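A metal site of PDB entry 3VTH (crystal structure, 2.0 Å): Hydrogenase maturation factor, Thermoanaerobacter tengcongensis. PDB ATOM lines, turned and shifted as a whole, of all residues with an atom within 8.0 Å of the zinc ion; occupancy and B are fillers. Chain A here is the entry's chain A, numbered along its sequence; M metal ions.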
ATOM      1  N   LEU A  74      20.364  11.190   4.525  1.00  0.00           N
ATOM      2  CA  LEU A  74      21.248  12.346   4.735  1.00  0.00           C
ATOM      3  C   LEU A  74      20.784  13.290   5.846  1.00  0.00           C
ATOM      4  O   LEU A  74      21.475  14.251   6.164  1.00  0.00           O
ATOM      5  CB  LEU A  74      21.437  13.134   3.441  1.00  0.00           C
ATOM      6  CG  LEU A  74      22.098  12.439   2.249  1.00  0.00           C
ATOM      7  CD1 LEU A  74      22.245  13.495   1.120  1.00  0.00           C
ATOM      8  CD2 LEU A  74      23.455  11.809   2.601  1.00  0.00           C
ATOM      9  N   MET A 111      27.966  15.433  -0.520  1.00  0.00           N
ATOM     10  CA  MET A 111      27.957  13.984  -0.302  1.00  0.00           C
ATOM     11  C   MET A 111      28.399  13.187  -1.526  1.00  0.00           C
ATOM     12  O   MET A 111      28.047  13.538  -2.659  1.00  0.00           O
ATOM     13  CB  MET A 111      26.562  13.526   0.164  1.00  0.00           C
ATOM     14  CG  MET A 111      26.211  13.969   1.600  1.00  0.00           C
ATOM     15  SD  MET A 111      27.240  13.170   2.861  1.00  0.00           S
ATOM     16  CE  MET A 111      27.057  14.299   4.248  1.00  0.00           C
ATOM     17  N   GLY A 112      29.174  12.121  -1.296  1.00  0.00           N
ATOM     18  CA  GLY A 112      29.581  11.158  -2.325  1.00  0.00           C
ATOM     19  C   GLY A 112      28.398  10.436  -2.967  1.00  0.00           C
ATOM     20  O   GLY A 112      27.315  10.343  -2.381  1.00  0.00           O
ATOM     21  N   VAL A 113      28.613   9.945  -4.192  1.00  0.00           N
ATOM     22  CA  VAL A 113      27.606   9.245  -4.992  1.00  0.00           C
ATOM     23  C   VAL A 113      27.018   8.061  -4.202  1.00  0.00           C
ATOM     24  O   VAL A 113      27.764   7.257  -3.633  1.00  0.00           O
ATOM     25  CB  VAL A 113      28.220   8.714  -6.312  1.00  0.00           C
ATOM     26  CG1 VAL A 113      27.139   8.123  -7.225  1.00  0.00           C
ATOM     27  CG2 VAL A 113      28.995   9.830  -7.037  1.00  0.00           C
ATOM     28  N   CYS A 114      25.689   7.984  -4.153  1.00  0.00           N
ATOM     29  CA  CYS A 114      25.007   6.865  -3.495  1.00  0.00           C
ATOM     30  C   CYS A 114      25.033   5.606  -4.363  1.00  0.00           C
ATOM     31  O   CYS A 114      25.327   5.676  -5.559  1.00  0.00           O
ATOM     32  CB  CYS A 114      23.550   7.233  -3.127  1.00  0.00           C
ATOM     33  SG  CYS A 114      22.408   7.323  -4.525  1.00  0.00           S
ATOM     34  N   GLU A 115      24.733   4.464  -3.769  1.00  0.00           N
ATOM     35  CA  GLU A 115      24.748   3.215  -4.535  1.00  0.00           C
ATOM     36  C   GLU A 115      23.707   3.152  -5.672  1.00  0.00           C
ATOM     37  O   GLU A 115      23.954   2.522  -6.687  1.00  0.00           O
ATOM     38  CB  GLU A 115      24.649   1.991  -3.614  1.00  0.00           C
ATOM     39  CG  GLU A 115      23.252   1.691  -3.073  1.00  0.00           C
ATOM     40  CD  GLU A 115      23.183   0.379  -2.297  1.00  0.00           C
ATOM     41  OE1 GLU A 115      23.381  -0.712  -2.902  1.00  0.00           O
ATOM     42  OE2 GLU A 115      22.924   0.424  -1.080  1.00  0.00           O
ATOM     43  N   ASP A 116      22.563   3.811  -5.505  1.00  0.00           N
ATOM     44  CA  ASP A 116      21.535   3.827  -6.573  1.00  0.00           C
ATOM     45  C   ASP A 116      21.988   4.635  -7.787  1.00  0.00           C
ATOM     46  O   ASP A 116      21.788   4.197  -8.910  1.00  0.00           O
ATOM     47  CB  ASP A 116      20.191   4.388  -6.070  1.00  0.00           C
ATOM     48  CG  ASP A 116      19.548   3.497  -5.011  1.00  0.00           C
ATOM     49  OD1 ASP A 116      19.415   2.296  -5.242  1.00  0.00           O
ATOM     50  OD2 ASP A 116      19.196   4.014  -3.932  1.00  0.00           O
ATOM     51  N   CYS A 117      22.574   5.802  -7.561  1.00  0.00           N
ATOM     52  CA  CYS A 117      23.097   6.603  -8.670  1.00  0.00           C
ATOM     53  C   CYS A 117      24.251   5.890  -9.371  1.00  0.00           C
ATOM     54  O   CYS A 117      24.357   5.942 -10.583  1.00  0.00           O
ATOM     55  CB  CYS A 117      23.540   8.001  -8.200  1.00  0.00           C
ATOM     56  SG  CYS A 117      22.138   9.100  -7.846  1.00  0.00           S
ATOM     57  N   LEU A 118      25.108   5.241  -8.586  1.00  0.00           N
ATOM     58  CA  LEU A 118      26.234   4.509  -9.141  1.00  0.00           C
ATOM     59  C   LEU A 118      25.770   3.364 -10.052  1.00  0.00           C
ATOM     60  O   LEU A 118      26.366   3.133 -11.103  1.00  0.00           O
ATOM     61  CB  LEU A 118      27.150   3.985  -8.032  1.00  0.00           C
ATOM     62  CG  LEU A 118      28.489   3.355  -8.447  1.00  0.00           C
ATOM     63  CD1 LEU A 118      29.342   4.359  -9.198  1.00  0.00           C
ATOM     64  CD2 LEU A 118      29.247   2.842  -7.213  1.00  0.00           C
ATOM     65  N   GLU A 120      22.864   3.283 -11.703  1.00  0.00           N
ATOM     66  CA  GLU A 120      22.354   3.960 -12.911  1.00  0.00           C
ATOM     67  C   GLU A 120      23.495   4.451 -13.816  1.00  0.00           C
ATOM     68  O   GLU A 120      23.461   4.223 -15.026  1.00  0.00           O
ATOM     69  CB  GLU A 120      21.412   5.110 -12.529  1.00  0.00           C
ATOM     70  CG  GLU A 120      20.049   4.636 -11.945  1.00  0.00           C
ATOM     71  CD  GLU A 120      19.189   5.767 -11.372  1.00  0.00           C
ATOM     72  OE1 GLU A 120      18.082   5.483 -10.872  1.00  0.00           O
ATOM     73  OE2 GLU A 120      19.620   6.936 -11.380  1.00  0.00           O
ATOM     74  N   ILE A 134      25.327  12.874 -12.416  1.00  0.00           N
ATOM     75  CA  ILE A 134      24.260  12.104 -11.782  1.00  0.00           C
ATOM     76  C   ILE A 134      24.232  12.327 -10.262  1.00  0.00           C
ATOM     77  O   ILE A 134      25.270  12.272  -9.608  1.00  0.00           O
ATOM     78  CB  ILE A 134      24.325  10.613 -12.166  1.00  0.00           C
ATOM     79  CG1 ILE A 134      23.049   9.876 -11.723  1.00  0.00           C
ATOM     80  CG2 ILE A 134      25.621   9.945 -11.626  1.00  0.00           C
ATOM     81  CD1 ILE A 134      22.911   8.468 -12.376  1.00  0.00           C
ATOM     82  N   ASN A 135      23.045  12.624  -9.730  1.00  0.00           N
ATOM     83  CA  ASN A 135      22.830  12.713  -8.279  1.00  0.00           C
ATOM     84  C   ASN A 135      21.349  12.468  -7.994  1.00  0.00           C
ATOM     85  O   ASN A 135      20.576  12.223  -8.917  1.00  0.00           O
ATOM     86  CB  ASN A 135      23.275  14.077  -7.721  1.00  0.00           C
ATOM     87  CG  ASN A 135      22.614  15.256  -8.450  1.00  0.00           C
ATOM     88  OD1 ASN A 135      21.499  15.148  -8.994  1.00  0.00           O
ATOM     89  ND2 ASN A 135      23.284  16.390  -8.458  1.00  0.00           N
ATOM     90  N   CYS A 136      20.946  12.545  -6.727  1.00  0.00           N
ATOM     91  CA  CYS A 136      19.553  12.350  -6.339  1.00  0.00           C
ATOM     92  C   CYS A 136      19.387  12.977  -4.955  1.00  0.00           C
ATOM     93  O   CYS A 136      20.291  13.663  -4.486  1.00  0.00           O
ATOM     94  CB  CYS A 136      19.213  10.850  -6.319  1.00  0.00           C
ATOM     95  SG  CYS A 136      20.027   9.898  -5.004  1.00  0.00           S
ATOM     96  N   THR A 137      18.235  12.774  -4.315  1.00  0.00           N
ATOM     97  CA  THR A 137      18.010  13.346  -2.980  1.00  0.00           C
ATOM     98  C   THR A 137      18.992  12.814  -1.928  1.00  0.00           C
ATOM     99  O   THR A 137      19.165  13.459  -0.891  1.00  0.00           O
ATOM    100  CB  THR A 137      16.553  13.124  -2.468  1.00  0.00           C
ATOM    101  OG1 THR A 137      16.281  11.724  -2.345  1.00  0.00           O
ATOM    102  CG2 THR A 137      15.560  13.732  -3.420  1.00  0.00           C
ATOM    103  N   ASN A 138      19.632  11.675  -2.199  1.00  0.00           N
ATOM    104  CA  ASN A 138      20.507  11.014  -1.225  1.00  0.00           C
ATOM    105  C   ASN A 138      22.034  11.204  -1.419  1.00  0.00           C
ATOM    106  O   ASN A 138      22.827  10.577  -0.691  1.00  0.00           O
ATOM    107  CB  ASN A 138      20.214   9.497  -1.172  1.00  0.00           C
ATOM    108  CG  ASN A 138      18.809   9.176  -0.687  1.00  0.00           C
ATOM    109  OD1 ASN A 138      18.308   9.787   0.257  1.00  0.00           O
ATOM    110  ND2 ASN A 138      18.177   8.192  -1.321  1.00  0.00           N
ATOM    111  N   CYS A 139      22.438  12.027  -2.397  1.00  0.00           N
ATOM    112  CA  CYS A 139      23.858  12.212  -2.739  1.00  0.00           C
ATOM    113  C   CYS A 139      24.113  13.466  -3.572  1.00  0.00           C
ATOM    114  O   CYS A 139      23.165  14.099  -4.045  1.00  0.00           O
ATOM    115  CB  CYS A 139      24.407  10.981  -3.487  1.00  0.00           C
ATOM    116  SG  CYS A 139      23.975  10.843  -5.263  1.00  0.00           S
ATOM    117  N   GLY A 140      25.379  13.831  -3.733  1.00  0.00           N
ATOM    118  CA  GLY A 140      25.771  14.953  -4.594  1.00  0.00           C
ATOM    119  C   GLY A 140      26.129  16.210  -3.815  1.00  0.00           C
ATOM    120  O   GLY A 140      26.115  16.234  -2.573  1.00  0.00           O
ATOM    121  N   ARG A 142      25.909  19.800  -2.056  1.00  0.00           N
ATOM    122  CA  ARG A 142      24.899  20.516  -1.297  1.00  0.00           C
ATOM    123  C   ARG A 142      25.517  21.867  -0.971  1.00  0.00           C
ATOM    124  O   ARG A 142      25.417  22.797  -1.761  1.00  0.00           O
ATOM    125  CB  ARG A 142      24.461  19.740  -0.046  1.00  0.00           C
ATOM    126  CG  ARG A 142      23.660  18.431  -0.318  1.00  0.00           C
ATOM    127  CD  ARG A 142      22.328  18.695  -1.068  1.00  0.00           C
ATOM    128  NE  ARG A 142      21.560  17.446  -1.171  1.00  0.00           N
ATOM    129  CZ  ARG A 142      21.675  16.554  -2.149  1.00  0.00           C
ATOM    130  NH1 ARG A 142      22.532  16.739  -3.143  1.00  0.00           N
ATOM    131  NH2 ARG A 142      20.936  15.442  -2.124  1.00  0.00           N
ATOM    132  N   ARG A 177      12.019   7.594  -8.078  1.00  0.00           N
ATOM    133  CA  ARG A 177      12.850   7.867  -6.916  1.00  0.00           C
ATOM    134  C   ARG A 177      13.368   9.299  -6.916  1.00  0.00           C
ATOM    135  O   ARG A 177      13.821   9.789  -5.868  1.00  0.00           O
ATOM    136  CB  ARG A 177      13.968   6.828  -6.746  1.00  0.00           C
ATOM    137  CG  ARG A 177      15.164   7.007  -7.641  1.00  0.00           C
ATOM    138  CD  ARG A 177      16.202   5.936  -7.329  1.00  0.00           C
ATOM    139  NE  ARG A 177      17.477   6.276  -7.946  1.00  0.00           N
ATOM    140  CZ  ARG A 177      18.412   7.012  -7.361  1.00  0.00           C
ATOM    141  NH1 ARG A 177      18.237   7.474  -6.128  1.00  0.00           N
ATOM    142  NH2 ARG A 177      19.531   7.263  -7.997  1.00  0.00           N
ATOM    143  N   ARG A 178      13.267   9.970  -8.064  1.00  0.00           N
ATOM    144  CA  ARG A 178      13.612  11.407  -8.155  1.00  0.00           C
ATOM    145  C   ARG A 178      12.397  12.344  -8.046  1.00  0.00           C
ATOM    146  O   ARG A 178      12.486  13.512  -8.417  1.00  0.00           O
ATOM    147  CB  ARG A 178      14.418  11.709  -9.425  1.00  0.00           C
ATOM    148  CG  ARG A 178      15.847  11.239  -9.343  1.00  0.00           C
ATOM    149  CD  ARG A 178      16.616  11.532 -10.635  1.00  0.00           C
ATOM    150  NE  ARG A 178      18.010  11.111 -10.490  1.00  0.00           N
ATOM    151  CZ  ARG A 178      18.449   9.884 -10.759  1.00  0.00           C
ATOM    152  NH1 ARG A 178      17.608   8.947 -11.195  1.00  0.00           N
ATOM    153  NH2 ARG A 178      19.736   9.610 -10.578  1.00  0.00           N
ATOM    154  N   GLN A 279      29.753   8.279   2.713  1.00  0.00           N
ATOM    155  CA  GLN A 279      29.456   9.308   1.702  1.00  0.00           C
ATOM    156  C   GLN A 279      30.164  10.635   1.986  1.00  0.00           C
ATOM    157  O   GLN A 279      30.312  11.470   1.096  1.00  0.00           O
ATOM    158  CB  GLN A 279      27.949   9.552   1.578  1.00  0.00           C
ATOM    159  CG  GLN A 279      27.206   8.547   0.712  1.00  0.00           C
ATOM    160  CD  GLN A 279      25.748   8.914   0.612  1.00  0.00           C
ATOM    161  OE1 GLN A 279      24.971   8.636   1.534  1.00  0.00           O
ATOM    162  NE2 GLN A 279      25.358   9.571  -0.473  1.00  0.00           N
HETATM  163 ZN    ZN M   1      22.220   9.370  -5.571  1.00  0.00          ZN
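Four residues have an atom within 4 Å of the zinc ion: Cys 114, Cys 117, Cys 136 and Cys 139. Along chain A the residues within 4 Å of the zinc ion span positions 114 to 139.
O of Asn 135 sits close to SG of Cys 117 (3.7 Å). SG of Cys 136 sits close to NH1 of Arg 177 (3.2 Å). The side-chain sulfur (SG) of Cys 114 sits close to the backbone NH (N) of Asp 116 (3.6 Å). The guanidinium group (NH1) of Arg 142 sits at hydrogen-bond distance from the backbone carbonyl oxygen (O) of Cys 139. O of Cys 136 sits at hydrogen-bond distance from NH2 of Arg 142 (3.0 Å). The side-chain sulfur (SG) of Cys 136 lies close to the backbone NH (N) of Asn 138 (3.3 Å). The guanidinium group (NH2) of Arg 178 lies close to the side-chain sulfur (SG) of Cys 117 (3.7 Å). NH2 of Arg 177 lies close to SG of Cys 117 (3.2 Å).
The zinc ion is bound by the side-chain sulfur (SG) of Cys 117 (2.3 Å), the side-chain sulfur (SG) of Cys 114 (2.3 Å), the side-chain sulfur (SG) of Cys 139 (2.3 Å) and the side-chain sulfur (SG) of Cys 136 (2.3 Å). The zinc ion has four donor atoms within binding distance.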
